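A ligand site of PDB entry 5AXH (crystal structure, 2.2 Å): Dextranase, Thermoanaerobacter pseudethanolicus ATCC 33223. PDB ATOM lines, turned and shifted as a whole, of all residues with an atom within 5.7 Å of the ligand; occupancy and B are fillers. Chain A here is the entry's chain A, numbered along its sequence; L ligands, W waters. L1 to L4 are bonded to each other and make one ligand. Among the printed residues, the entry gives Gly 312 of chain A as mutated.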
ATOM      1  N   TYR A 184      -8.410 -31.746 -23.692  1.00  0.00           N
ATOM      2  CA  TYR A 184      -7.537 -30.593 -23.760  1.00  0.00           C
ATOM      3  C   TYR A 184      -6.692 -30.500 -22.480  1.00  0.00           C
ATOM      4  O   TYR A 184      -7.227 -30.496 -21.388  1.00  0.00           O
ATOM      5  CB  TYR A 184      -8.378 -29.309 -23.898  1.00  0.00           C
ATOM      6  CG  TYR A 184      -7.551 -28.064 -24.096  1.00  0.00           C
ATOM      7  CD1 TYR A 184      -7.163 -27.647 -25.393  1.00  0.00           C
ATOM      8  CD2 TYR A 184      -7.116 -27.312 -23.009  1.00  0.00           C
ATOM      9  CE1 TYR A 184      -6.386 -26.508 -25.571  1.00  0.00           C
ATOM     10  CE2 TYR A 184      -6.350 -26.154 -23.205  1.00  0.00           C
ATOM     11  CZ  TYR A 184      -5.980 -25.756 -24.465  1.00  0.00           C
ATOM     12  OH  TYR A 184      -5.203 -24.616 -24.643  1.00  0.00           O
ATOM     13  N   ASP A 185      -5.375 -30.396 -22.630  1.00  0.00           N
ATOM     14  CA  ASP A 185      -4.432 -30.259 -21.500  1.00  0.00           C
ATOM     15  C   ASP A 185      -4.553 -31.361 -20.430  1.00  0.00           C
ATOM     16  O   ASP A 185      -4.480 -31.079 -19.221  1.00  0.00           O
ATOM     17  CB  ASP A 185      -4.490 -28.844 -20.915  1.00  0.00           C
ATOM     18  CG  ASP A 185      -3.795 -27.807 -21.785  1.00  0.00           C
ATOM     19  OD1 ASP A 185      -3.262 -28.161 -22.854  1.00  0.00           O
ATOM     20  OD2 ASP A 185      -3.744 -26.618 -21.383  1.00  0.00           O
ATOM     21  N   GLN A 187      -2.359 -34.021 -20.845  1.00  0.00           N
ATOM     22  CA  GLN A 187      -1.043 -34.635 -20.890  1.00  0.00           C
ATOM     23  C   GLN A 187      -0.038 -34.080 -19.839  1.00  0.00           C
ATOM     24  O   GLN A 187      -0.298 -33.064 -19.191  1.00  0.00           O
ATOM     25  CB  GLN A 187      -0.451 -34.530 -22.317  1.00  0.00           C
ATOM     26  CG  GLN A 187       0.147 -33.168 -22.662  1.00  0.00           C
ATOM     27  CD  GLN A 187       0.598 -33.056 -24.117  1.00  0.00           C
ATOM     28  OE1 GLN A 187       0.882 -34.052 -24.770  1.00  0.00           O
ATOM     29  NE2 GLN A 187       0.689 -31.810 -24.617  1.00  0.00           N
ATOM     30  N   HIS A 190       4.391 -31.589 -23.403  1.00  0.00           N
ATOM     31  CA  HIS A 190       4.194 -31.583 -24.857  1.00  0.00           C
ATOM     32  C   HIS A 190       5.203 -32.519 -25.594  1.00  0.00           C
ATOM     33  O   HIS A 190       4.885 -33.116 -26.648  1.00  0.00           O
ATOM     34  CB  HIS A 190       4.241 -30.136 -25.407  1.00  0.00           C
ATOM     35  CG  HIS A 190       2.994 -29.348 -25.157  1.00  0.00           C
ATOM     36  ND1 HIS A 190       2.513 -29.077 -23.895  1.00  0.00           N
ATOM     37  CD2 HIS A 190       2.103 -28.793 -26.018  1.00  0.00           C
ATOM     38  CE1 HIS A 190       1.397 -28.390 -23.987  1.00  0.00           C
ATOM     39  NE2 HIS A 190       1.122 -28.196 -25.263  1.00  0.00           N
ATOM     40  N   ILE A 208       0.405 -28.468 -18.215  1.00  0.00           N
ATOM     41  CA  ILE A 208       1.070 -27.233 -18.659  1.00  0.00           C
ATOM     42  C   ILE A 208       0.825 -26.044 -17.727  1.00  0.00           C
ATOM     43  O   ILE A 208       1.712 -25.248 -17.497  1.00  0.00           O
ATOM     44  CB  ILE A 208       0.665 -26.902 -20.144  1.00  0.00           C
ATOM     45  CG1 ILE A 208       1.445 -25.712 -20.740  1.00  0.00           C
ATOM     46  CG2 ILE A 208      -0.825 -26.598 -20.273  1.00  0.00           C
ATOM     47  CD1 ILE A 208       2.860 -26.014 -21.153  1.00  0.00           C
ATOM     48  N   TYR A 235      -5.124 -34.210 -27.233  1.00  0.00           N
ATOM     49  CA  TYR A 235      -4.540 -32.950 -27.688  1.00  0.00           C
ATOM     50  C   TYR A 235      -3.047 -32.955 -27.448  1.00  0.00           C
ATOM     51  O   TYR A 235      -2.602 -33.213 -26.334  1.00  0.00           O
ATOM     52  CB  TYR A 235      -5.144 -31.742 -26.960  1.00  0.00           C
ATOM     53  CG  TYR A 235      -4.454 -30.435 -27.299  1.00  0.00           C
ATOM     54  CD1 TYR A 235      -4.764 -29.730 -28.452  1.00  0.00           C
ATOM     55  CD2 TYR A 235      -3.459 -29.927 -26.469  1.00  0.00           C
ATOM     56  CE1 TYR A 235      -4.110 -28.545 -28.773  1.00  0.00           C
ATOM     57  CE2 TYR A 235      -2.809 -28.760 -26.762  1.00  0.00           C
ATOM     58  CZ  TYR A 235      -3.127 -28.064 -27.908  1.00  0.00           C
ATOM     59  OH  TYR A 235      -2.421 -26.893 -28.176  1.00  0.00           O
ATOM     60  N   LEU A 237       0.426 -30.413 -29.320  1.00  0.00           N
ATOM     61  CA  LEU A 237       1.005 -29.733 -30.470  1.00  0.00           C
ATOM     62  C   LEU A 237       1.833 -30.683 -31.343  1.00  0.00           C
ATOM     63  O   LEU A 237       2.349 -31.709 -30.889  1.00  0.00           O
ATOM     64  CB  LEU A 237       1.886 -28.567 -30.037  1.00  0.00           C
ATOM     65  CG  LEU A 237       1.211 -27.380 -29.388  1.00  0.00           C
ATOM     66  CD1 LEU A 237       2.274 -26.371 -29.000  1.00  0.00           C
ATOM     67  CD2 LEU A 237       0.187 -26.719 -30.312  1.00  0.00           C
ATOM     68  N   HIS A 268       6.126 -20.281 -27.662  1.00  0.00           N
ATOM     69  CA  HIS A 268       4.808 -19.826 -27.237  1.00  0.00           C
ATOM     70  C   HIS A 268       4.967 -19.440 -25.772  1.00  0.00           C
ATOM     71  O   HIS A 268       5.156 -20.320 -24.939  1.00  0.00           O
ATOM     72  CB  HIS A 268       3.769 -20.958 -27.390  1.00  0.00           C
ATOM     73  CG  HIS A 268       2.366 -20.544 -27.090  1.00  0.00           C
ATOM     74  ND1 HIS A 268       1.731 -19.534 -27.788  1.00  0.00           N
ATOM     75  CD2 HIS A 268       1.461 -21.018 -26.201  1.00  0.00           C
ATOM     76  CE1 HIS A 268       0.501 -19.386 -27.316  1.00  0.00           C
ATOM     77  NE2 HIS A 268       0.311 -20.287 -26.360  1.00  0.00           N
ATOM     78  N   PRO A 269       4.960 -18.118 -25.473  1.00  0.00           N
ATOM     79  CA  PRO A 269       5.126 -17.707 -24.074  1.00  0.00           C
ATOM     80  C   PRO A 269       3.912 -18.038 -23.224  1.00  0.00           C
ATOM     81  O   PRO A 269       2.783 -18.009 -23.720  1.00  0.00           O
ATOM     82  CB  PRO A 269       5.368 -16.183 -24.153  1.00  0.00           C
ATOM     83  CG  PRO A 269       4.874 -15.771 -25.499  1.00  0.00           C
ATOM     84  CD  PRO A 269       5.009 -16.975 -26.399  1.00  0.00           C
ATOM     85  N   LEU A 270       4.160 -18.342 -21.958  1.00  0.00           N
ATOM     86  CA  LEU A 270       3.107 -18.732 -21.045  1.00  0.00           C
ATOM     87  C   LEU A 270       3.245 -17.945 -19.748  1.00  0.00           C
ATOM     88  O   LEU A 270       4.340 -17.560 -19.410  1.00  0.00           O
ATOM     89  CB  LEU A 270       3.224 -20.222 -20.775  1.00  0.00           C
ATOM     90  CG  LEU A 270       3.080 -21.138 -21.981  1.00  0.00           C
ATOM     91  CD1 LEU A 270       3.493 -22.559 -21.599  1.00  0.00           C
ATOM     92  CD2 LEU A 270       1.665 -21.127 -22.519  1.00  0.00           C
ATOM     93  N   PRO A 271       2.125 -17.740 -19.016  1.00  0.00           N
ATOM     94  CA  PRO A 271       2.151 -17.097 -17.690  1.00  0.00           C
ATOM     95  C   PRO A 271       3.113 -17.776 -16.703  1.00  0.00           C
ATOM     96  O   PRO A 271       3.271 -18.996 -16.731  1.00  0.00           O
ATOM     97  CB  PRO A 271       0.717 -17.257 -17.181  1.00  0.00           C
ATOM     98  CG  PRO A 271      -0.115 -17.557 -18.362  1.00  0.00           C
ATOM     99  CD  PRO A 271       0.794 -18.290 -19.327  1.00  0.00           C
ATOM    100  N   TRP A 274       2.971 -21.217 -14.618  1.00  0.00           N
ATOM    101  CA  TRP A 274       2.717 -22.451 -15.376  1.00  0.00           C
ATOM    102  C   TRP A 274       3.941 -23.370 -15.305  1.00  0.00           C
ATOM    103  O   TRP A 274       4.977 -22.978 -14.756  1.00  0.00           O
ATOM    104  CB  TRP A 274       2.312 -22.110 -16.829  1.00  0.00           C
ATOM    105  CG  TRP A 274       0.899 -21.572 -16.905  1.00  0.00           C
ATOM    106  CD1 TRP A 274       0.267 -20.752 -15.999  1.00  0.00           C
ATOM    107  CD2 TRP A 274      -0.069 -21.816 -17.943  1.00  0.00           C
ATOM    108  NE1 TRP A 274      -1.017 -20.497 -16.407  1.00  0.00           N
ATOM    109  CE2 TRP A 274      -1.255 -21.132 -17.594  1.00  0.00           C
ATOM    110  CE3 TRP A 274      -0.057 -22.558 -19.131  1.00  0.00           C
ATOM    111  CZ2 TRP A 274      -2.391 -21.151 -18.393  1.00  0.00           C
ATOM    112  CZ3 TRP A 274      -1.187 -22.589 -19.911  1.00  0.00           C
ATOM    113  CH2 TRP A 274      -2.343 -21.883 -19.546  1.00  0.00           C
ATOM    114  N   LEU A 279       6.768 -22.769 -24.383  1.00  0.00           N
ATOM    115  CA  LEU A 279       6.903 -23.985 -25.174  1.00  0.00           C
ATOM    116  C   LEU A 279       7.829 -23.658 -26.308  1.00  0.00           C
ATOM    117  O   LEU A 279       7.541 -22.751 -27.062  1.00  0.00           O
ATOM    118  CB  LEU A 279       5.566 -24.448 -25.734  1.00  0.00           C
ATOM    119  CG  LEU A 279       4.633 -25.027 -24.683  1.00  0.00           C
ATOM    120  CD1 LEU A 279       3.222 -25.113 -25.247  1.00  0.00           C
ATOM    121  CD2 LEU A 279       5.121 -26.397 -24.226  1.00  0.00           C
ATOM    122  N   GLY A 312      -2.388 -30.103 -32.623  1.00  0.00           N
ATOM    123  CA  GLY A 312      -2.516 -28.663 -32.638  1.00  0.00           C
ATOM    124  C   GLY A 312      -1.384 -27.985 -33.396  1.00  0.00           C
ATOM    125  O   GLY A 312      -0.284 -28.543 -33.537  1.00  0.00           O
ATOM    126  N   THR A 313      -1.662 -26.776 -33.896  1.00  0.00           N
ATOM    127  CA  THR A 313      -0.629 -25.882 -34.412  1.00  0.00           C
ATOM    128  C   THR A 313      -0.910 -24.499 -33.867  1.00  0.00           C
ATOM    129  O   THR A 313      -1.957 -24.268 -33.289  1.00  0.00           O
ATOM    130  CB  THR A 313      -0.590 -25.792 -35.969  1.00  0.00           C
ATOM    131  OG1 THR A 313      -1.726 -25.066 -36.442  1.00  0.00           O
ATOM    132  CG2 THR A 313      -0.504 -27.179 -36.608  1.00  0.00           C
ATOM    133  N   LEU A 314       0.025 -23.578 -34.060  1.00  0.00           N
ATOM    134  CA  LEU A 314      -0.130 -22.221 -33.532  1.00  0.00           C
ATOM    135  C   LEU A 314      -0.366 -21.182 -34.626  1.00  0.00           C
ATOM    136  O   LEU A 314      -0.402 -19.985 -34.340  1.00  0.00           O
ATOM    137  CB  LEU A 314       1.127 -21.849 -32.718  1.00  0.00           C
ATOM    138  CG  LEU A 314       1.367 -22.745 -31.499  1.00  0.00           C
ATOM    139  CD1 LEU A 314       2.613 -22.269 -30.780  1.00  0.00           C
ATOM    140  CD2 LEU A 314       0.186 -22.714 -30.546  1.00  0.00           C
ATOM    141  N   ASN A 352      -5.368 -29.179 -36.404  1.00  0.00           N
ATOM    142  CA  ASN A 352      -5.900 -27.811 -36.356  1.00  0.00           C
ATOM    143  C   ASN A 352      -5.051 -26.838 -37.166  1.00  0.00           C
ATOM    144  O   ASN A 352      -3.959 -26.440 -36.734  1.00  0.00           O
ATOM    145  CB  ASN A 352      -6.013 -27.331 -34.914  1.00  0.00           C
ATOM    146  CG  ASN A 352      -6.386 -25.858 -34.787  1.00  0.00           C
ATOM    147  OD1 ASN A 352      -7.043 -25.269 -35.668  1.00  0.00           O
ATOM    148  ND2 ASN A 352      -5.954 -25.252 -33.694  1.00  0.00           N
ATOM    149  N   VAL A 354      -4.858 -23.350 -37.716  1.00  0.00           N
ATOM    150  CA  VAL A 354      -5.235 -22.042 -37.170  1.00  0.00           C
ATOM    151  C   VAL A 354      -5.318 -20.985 -38.261  1.00  0.00           C
ATOM    152  O   VAL A 354      -4.379 -20.829 -39.047  1.00  0.00           O
ATOM    153  CB  VAL A 354      -4.227 -21.513 -36.103  1.00  0.00           C
ATOM    154  CG1 VAL A 354      -4.653 -20.152 -35.582  1.00  0.00           C
ATOM    155  CG2 VAL A 354      -4.122 -22.484 -34.935  1.00  0.00           C
ATOM    156  N   TYR A 372     -10.067 -29.215 -39.360  1.00  0.00           N
ATOM    157  CA  TYR A 372     -10.341 -28.454 -38.146  1.00  0.00           C
ATOM    158  C   TYR A 372      -9.681 -27.079 -38.272  1.00  0.00           C
ATOM    159  O   TYR A 372      -8.454 -26.969 -38.437  1.00  0.00           O
ATOM    160  CB  TYR A 372      -9.822 -29.228 -36.939  1.00  0.00           C
ATOM    161  CG  TYR A 372     -10.150 -28.667 -35.568  1.00  0.00           C
ATOM    162  CD1 TYR A 372      -9.389 -27.622 -35.021  1.00  0.00           C
ATOM    163  CD2 TYR A 372     -11.165 -29.204 -34.789  1.00  0.00           C
ATOM    164  CE1 TYR A 372      -9.640 -27.116 -33.766  1.00  0.00           C
ATOM    165  CE2 TYR A 372     -11.437 -28.692 -33.514  1.00  0.00           C
ATOM    166  CZ  TYR A 372     -10.662 -27.655 -33.008  1.00  0.00           C
ATOM    167  OH  TYR A 372     -10.900 -27.163 -31.765  1.00  0.00           O
ATOM    168  N   GLU A 374      -9.477 -23.365 -36.408  1.00  0.00           N
ATOM    169  CA  GLU A 374      -9.657 -22.451 -35.304  1.00  0.00           C
ATOM    170  C   GLU A 374      -9.502 -21.038 -35.813  1.00  0.00           C
ATOM    171  O   GLU A 374      -8.505 -20.712 -36.445  1.00  0.00           O
ATOM    172  CB  GLU A 374      -8.620 -22.723 -34.215  1.00  0.00           C
ATOM    173  CG  GLU A 374      -8.733 -21.848 -32.971  1.00  0.00           C
ATOM    174  CD  GLU A 374      -7.628 -22.109 -31.946  1.00  0.00           C
ATOM    175  OE1 GLU A 374      -6.487 -22.428 -32.330  1.00  0.00           O
ATOM    176  OE2 GLU A 374      -7.856 -21.952 -30.737  1.00  0.00           O
ATOM    177  N   TRP A 376      -8.665 -17.368 -34.666  1.00  0.00           N
ATOM    178  CA  TRP A 376      -8.263 -16.402 -33.668  1.00  0.00           C
ATOM    179  C   TRP A 376      -8.673 -15.024 -34.220  1.00  0.00           C
ATOM    180  O   TRP A 376      -8.665 -14.830 -35.437  1.00  0.00           O
ATOM    181  CB  TRP A 376      -6.754 -16.460 -33.426  1.00  0.00           C
ATOM    182  CG  TRP A 376      -6.256 -17.707 -32.725  1.00  0.00           C
ATOM    183  CD1 TRP A 376      -7.016 -18.695 -32.176  1.00  0.00           C
ATOM    184  CD2 TRP A 376      -4.879 -18.064 -32.460  1.00  0.00           C
ATOM    185  NE1 TRP A 376      -6.206 -19.665 -31.622  1.00  0.00           N
ATOM    186  CE2 TRP A 376      -4.899 -19.301 -31.761  1.00  0.00           C
ATOM    187  CE3 TRP A 376      -3.644 -17.471 -32.748  1.00  0.00           C
ATOM    188  CZ2 TRP A 376      -3.730 -19.956 -31.345  1.00  0.00           C
ATOM    189  CZ3 TRP A 376      -2.474 -18.125 -32.342  1.00  0.00           C
ATOM    190  CH2 TRP A 376      -2.523 -19.360 -31.634  1.00  0.00           C
ATOM    191  N   TYR A 408     -14.841 -18.963 -31.019  1.00  0.00           N
ATOM    192  CA  TYR A 408     -15.161 -18.839 -29.598  1.00  0.00           C
ATOM    193  C   TYR A 408     -16.124 -17.676 -29.409  1.00  0.00           C
ATOM    194  O   TYR A 408     -15.785 -16.540 -29.697  1.00  0.00           O
ATOM    195  CB  TYR A 408     -13.889 -18.625 -28.758  1.00  0.00           C
ATOM    196  CG  TYR A 408     -12.842 -19.660 -29.032  1.00  0.00           C
ATOM    197  CD1 TYR A 408     -13.104 -21.009 -28.824  1.00  0.00           C
ATOM    198  CD2 TYR A 408     -11.617 -19.303 -29.583  1.00  0.00           C
ATOM    199  CE1 TYR A 408     -12.141 -21.980 -29.114  1.00  0.00           C
ATOM    200  CE2 TYR A 408     -10.653 -20.260 -29.870  1.00  0.00           C
ATOM    201  CZ  TYR A 408     -10.928 -21.597 -29.641  1.00  0.00           C
ATOM    202  OH  TYR A 408      -9.980 -22.567 -29.932  1.00  0.00           O
ATOM    203  N   ASP A 415     -13.438 -12.642 -20.197  1.00  0.00           N
ATOM    204  CA  ASP A 415     -12.863 -12.399 -18.850  1.00  0.00           C
ATOM    205  C   ASP A 415     -13.878 -11.870 -17.844  1.00  0.00           C
ATOM    206  O   ASP A 415     -13.504 -11.556 -16.732  1.00  0.00           O
ATOM    207  CB  ASP A 415     -11.677 -11.433 -18.927  1.00  0.00           C
ATOM    208  CG  ASP A 415     -10.531 -11.981 -19.744  1.00  0.00           C
ATOM    209  OD1 ASP A 415     -10.280 -13.211 -19.687  1.00  0.00           O
ATOM    210  OD2 ASP A 415      -9.880 -11.190 -20.455  1.00  0.00           O
ATOM    211  N   LYS A 450     -12.944 -19.264 -24.931  1.00  0.00           N
ATOM    212  CA  LYS A 450     -11.613 -18.893 -25.423  1.00  0.00           C
ATOM    213  C   LYS A 450     -10.711 -20.068 -25.709  1.00  0.00           C
ATOM    214  O   LYS A 450     -11.045 -21.214 -25.412  1.00  0.00           O
ATOM    215  CB  LYS A 450     -10.928 -17.903 -24.463  1.00  0.00           C
ATOM    216  CG  LYS A 450     -11.027 -18.223 -22.999  1.00  0.00           C
ATOM    217  CD  LYS A 450     -10.957 -16.951 -22.175  1.00  0.00           C
ATOM    218  CE  LYS A 450      -9.658 -16.204 -22.353  1.00  0.00           C
ATOM    219  NZ  LYS A 450      -9.494 -15.220 -21.256  1.00  0.00           N
ATOM    220  N   GLU A 451      -9.591 -19.782 -26.360  1.00  0.00           N
ATOM    221  CA  GLU A 451      -8.698 -20.823 -26.869  1.00  0.00           C
ATOM    222  C   GLU A 451      -8.145 -21.714 -25.760  1.00  0.00           C
ATOM    223  O   GLU A 451      -7.850 -22.887 -26.025  1.00  0.00           O
ATOM    224  CB  GLU A 451      -7.567 -20.247 -27.746  1.00  0.00           C
ATOM    225  CG  GLU A 451      -6.475 -19.469 -27.048  1.00  0.00           C
ATOM    226  CD  GLU A 451      -6.756 -17.989 -26.894  1.00  0.00           C
ATOM    227  OE1 GLU A 451      -7.935 -17.600 -26.724  1.00  0.00           O
ATOM    228  OE2 GLU A 451      -5.771 -17.241 -26.909  1.00  0.00           O
ATOM    229  N   TYR A 452      -7.997 -21.168 -24.544  1.00  0.00           N
ATOM    230  CA  TYR A 452      -7.670 -21.950 -23.371  1.00  0.00           C
ATOM    231  C   TYR A 452      -8.963 -22.588 -22.861  1.00  0.00           C
ATOM    232  O   TYR A 452      -9.711 -21.971 -22.128  1.00  0.00           O
ATOM    233  CB  TYR A 452      -7.005 -21.081 -22.280  1.00  0.00           C
ATOM    234  CG  TYR A 452      -6.591 -21.899 -21.078  1.00  0.00           C
ATOM    235  CD1 TYR A 452      -5.671 -22.935 -21.218  1.00  0.00           C
ATOM    236  CD2 TYR A 452      -7.109 -21.646 -19.811  1.00  0.00           C
ATOM    237  CE1 TYR A 452      -5.288 -23.712 -20.153  1.00  0.00           C
ATOM    238  CE2 TYR A 452      -6.735 -22.421 -18.705  1.00  0.00           C
ATOM    239  CZ  TYR A 452      -5.820 -23.455 -18.896  1.00  0.00           C
ATOM    240  OH  TYR A 452      -5.430 -24.249 -17.864  1.00  0.00           O
ATOM    241  N   PHE A 453      -9.207 -23.842 -23.256  1.00  0.00           N
ATOM    242  CA  PHE A 453     -10.519 -24.503 -23.024  1.00  0.00           C
ATOM    243  C   PHE A 453     -11.002 -24.537 -21.579  1.00  0.00           C
ATOM    244  O   PHE A 453     -12.186 -24.389 -21.348  1.00  0.00           O
ATOM    245  CB  PHE A 453     -10.521 -25.933 -23.565  1.00  0.00           C
ATOM    246  CG  PHE A 453     -10.640 -26.053 -25.055  1.00  0.00           C
ATOM    247  CD1 PHE A 453     -10.315 -25.017 -25.919  1.00  0.00           C
ATOM    248  CD2 PHE A 453     -11.030 -27.278 -25.607  1.00  0.00           C
ATOM    249  CE1 PHE A 453     -10.429 -25.172 -27.293  1.00  0.00           C
ATOM    250  CE2 PHE A 453     -11.137 -27.440 -26.981  1.00  0.00           C
ATOM    251  CZ  PHE A 453     -10.834 -26.386 -27.814  1.00  0.00           C
ATOM    252  N   SER A 455     -10.833 -22.203 -19.437  1.00  0.00           N
ATOM    253  CA  SER A 455     -11.397 -20.903 -19.016  1.00  0.00           C
ATOM    254  C   SER A 455     -12.912 -20.925 -19.170  1.00  0.00           C
ATOM    255  O   SER A 455     -13.405 -21.105 -20.268  1.00  0.00           O
ATOM    256  CB  SER A 455     -10.798 -19.759 -19.814  1.00  0.00           C
ATOM    257  OG  SER A 455     -11.374 -18.545 -19.388  1.00  0.00           O
HETATM  258  C1  LIG L   1      -3.911 -24.823 -30.096  1.00  0.00           C
HETATM  259  C2  LIG L   1      -5.417 -24.776 -29.772  1.00  0.00           C
HETATM  260  C3  LIG L   1      -5.816 -23.750 -28.715  1.00  0.00           C
HETATM  261  C4  LIG L   1      -4.660 -23.502 -27.745  1.00  0.00           C
HETATM  262  C5  LIG L   1      -3.475 -22.918 -28.535  1.00  0.00           C
HETATM  263  C6  LIG L   1      -2.226 -22.712 -27.678  1.00  0.00           C
HETATM  264  O1  LIG L   1      -3.706 -25.068 -31.494  1.00  0.00           O
HETATM  265  O2  LIG L   1      -6.255 -24.584 -30.912  1.00  0.00           O
HETATM  266  O3  LIG L   1      -6.972 -24.329 -28.094  1.00  0.00           O
HETATM  267  O4  LIG L   1      -5.030 -22.593 -26.695  1.00  0.00           O
HETATM  268  O5  LIG L   1      -3.106 -23.701 -29.686  1.00  0.00           O
HETATM  269  O6  LIG L   1      -1.881 -23.967 -27.080  1.00  0.00           O
HETATM  270  C1  LG2 L   2      -0.709 -23.882 -26.268  1.00  0.00           C
HETATM  271  C2  LG2 L   2      -0.472 -25.252 -25.645  1.00  0.00           C
HETATM  272  C3  LG2 L   2      -1.630 -25.624 -24.716  1.00  0.00           C
HETATM  273  C4  LG2 L   2      -1.894 -24.499 -23.695  1.00  0.00           C
HETATM  274  C5  LG2 L   2      -1.951 -23.144 -24.390  1.00  0.00           C
HETATM  275  C6  LG2 L   2      -2.023 -21.987 -23.432  1.00  0.00           C
HETATM  276  O1  LG2 L   2      -0.314 -26.203 -26.685  1.00  0.00           O
HETATM  277  O2  LG2 L   2      -1.380 -26.874 -24.042  1.00  0.00           O
HETATM  278  O3  LG2 L   2      -3.152 -24.636 -23.059  1.00  0.00           O
HETATM  279  O4  LG2 L   2      -0.815 -22.916 -25.222  1.00  0.00           O
HETATM  280  O5  LG2 L   2      -1.863 -20.818 -24.244  1.00  0.00           O
HETATM  281  C1  LG3 L   3      -3.086 -20.095 -24.389  1.00  0.00           C
HETATM  282  C2  LG3 L   3      -2.813 -18.793 -25.131  1.00  0.00           C
HETATM  283  C3  LG3 L   3      -1.838 -17.940 -24.327  1.00  0.00           C
HETATM  284  C4  LG3 L   3      -2.454 -17.686 -22.955  1.00  0.00           C
HETATM  285  C5  LG3 L   3      -2.819 -19.014 -22.294  1.00  0.00           C
HETATM  286  C6  LG3 L   3      -3.513 -18.830 -20.969  1.00  0.00           C
HETATM  287  O1  LG3 L   3      -2.317 -19.126 -26.423  1.00  0.00           O
HETATM  288  O2  LG3 L   3      -1.627 -16.678 -24.918  1.00  0.00           O
HETATM  289  O3  LG3 L   3      -1.571 -16.987 -22.112  1.00  0.00           O
HETATM  290  O4  LG3 L   3      -3.689 -19.779 -23.137  1.00  0.00           O
HETATM  291  O5  LG3 L   3      -4.575 -17.871 -21.043  1.00  0.00           O
HETATM  292  C1  LG4 L   4      -4.756 -17.248 -19.754  1.00  0.00           C
HETATM  293  C2  LG4 L   4      -6.072 -16.482 -19.796  1.00  0.00           C
HETATM  294  C3  LG4 L   4      -5.826 -15.145 -20.474  1.00  0.00           C
HETATM  295  C4  LG4 L   4      -4.744 -14.324 -19.759  1.00  0.00           C
HETATM  296  C5  LG4 L   4      -3.795 -15.146 -18.857  1.00  0.00           C
HETATM  297  C6  LG4 L   4      -4.236 -15.341 -17.385  1.00  0.00           C
HETATM  298  O1  LG4 L   4      -7.066 -17.231 -20.523  1.00  0.00           O
HETATM  299  O2  LG4 L   4      -7.036 -14.397 -20.521  1.00  0.00           O
HETATM  300  O3  LG4 L   4      -4.014 -13.652 -20.799  1.00  0.00           O
HETATM  301  O4  LG4 L   4      -3.607 -16.433 -19.433  1.00  0.00           O
HETATM  302  O5  LG4 L   4      -3.331 -14.724 -16.462  1.00  0.00           O
HETATM  303  O   HOH W   1      -1.324 -30.151 -23.044  1.00  0.00           O
HETATM  304  O   HOH W   2      -3.314 -12.132 -16.217  1.00  0.00           O
HETATM  305  O   HOH W   3      -7.837 -27.114 -28.874  1.00  0.00           O
HETATM  306  O   HOH W   4      -6.599 -27.435 -31.404  1.00  0.00           O
HETATM  307  O   HOH W   5      -6.054 -18.110 -23.353  1.00  0.00           O
HETATM  308  O   HOH W   6      -9.325 -25.044 -30.997  1.00  0.00           O
HETATM  309  O   HOH W   7      -3.491 -17.729 -28.799  1.00  0.00           O
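O2 of LG2 L2 sits at hydrogen-bond distance from OD1 of Asp 185 (2.6 Å).
O2 of LIG L1 is in hydrogen-bond range of OE1 of Glu 374, at 2.6 Å.
OH of Tyr 184 sits at hydrogen-bond distance from O3 of LG2 L2.
The backbone carbonyl oxygen (O) of Thr 313 sits at hydrogen-bond distance from an oxygen (O1) of LIG L1.
The backbone carbonyl oxygen (O) of Glu 451 lies within hydrogen-bond range of an oxygen (O3) of LIG L1, 2.7 Å away.
The side-chain hydroxyl (OH) of Tyr 235 is in hydrogen-bond range of an oxygen (O1) of LG2 L2 (2.7 Å).
NZ of Lys 450 lies within hydrogen-bond range of O2 of LG4 L4, at 2.7 Å.
An oxygen (O1) of LG2 L2 sits at hydrogen-bond distance from a ring nitrogen (NE2) of His 190 (2.8 Å).
An oxygen (O1) of LG3 L3 lies within hydrogen-bond range of a ring nitrogen (NE2) of His 268 (2.9 Å).
ND2 of Asn 352 lies within hydrogen-bond range of O2 of LIG L1 (2.9 Å).
OD1 of Asn 352 is in hydrogen-bond range of N of Glu 374 (3.2 Å).
The side-chain carboxylate of Glu 374 sits close to the indole nitrogen of Trp 376.
The side-chain hydroxyl (OH) of Tyr 184 sits at hydrogen-bond distance from the backbone carbonyl oxygen (O) of Glu 451 (3.5 Å).
The side-chain hydroxyl (OG1) of Thr 313 sits at hydrogen-bond distance from the backbone carbonyl oxygen (O) of Asn 352 (2.6 Å).
The side-chain amino group (NZ) of Lys 450 is in salt-bridge range of the side-chain carboxylate (OD1) of Asp 415, at 2.7 Å.
The side-chain amide nitrogen (NE2) of Gln 187 sits at hydrogen-bond distance from a ring nitrogen (ND1) of His 190.
N of His 268 lies within hydrogen-bond range of O of Leu 279 (2.9 Å).
Water W4 bridges O2 of LIG L1 (2.9 Å) and ND2 of Asn 352 (3.2 Å).
Water W7 lies within hydrogen-bond range of O1 of LG3 L3 and OE2 of Glu 451.
Water W6 lies within hydrogen-bond range of OH of Tyr 372 (2.7 Å), OH of Tyr 408 (2.8 Å), O2 of LIG L1 (3.1 Å) and OE2 of Glu 374 (3.4 Å).
Water W1 lies within hydrogen-bond range of the side-chain carboxylate of Asp 185 (2.8 Å), the side-chain amide nitrogen of Gln 187 (3.0 Å) and an oxygen (O2) of LG2 L2 (3.4 Å).
Merely in contact with the ligand: Ile 208, Leu 237, Leu 270, Pro 271, Trp 274, Leu 279, Gly 312, Leu 314, Tyr 408, Asp 415, Tyr 452 and Phe 453.
22 residues have an atom within 4 Å of the ligand: Tyr 184, Asp 185, His 190, Ile 208, Tyr 235, Leu 237, His 268, Leu 270, Pro 271, Trp 274, Leu 279, Gly 312, Thr 313, Leu 314, Asn 352, Glu 374, Tyr 408, Asp 415, Lys 450, Glu 451, Tyr 452 and Phe 453.
The nearest printed residue that does not touch the ligand is Trp 376 (4.1 Å).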
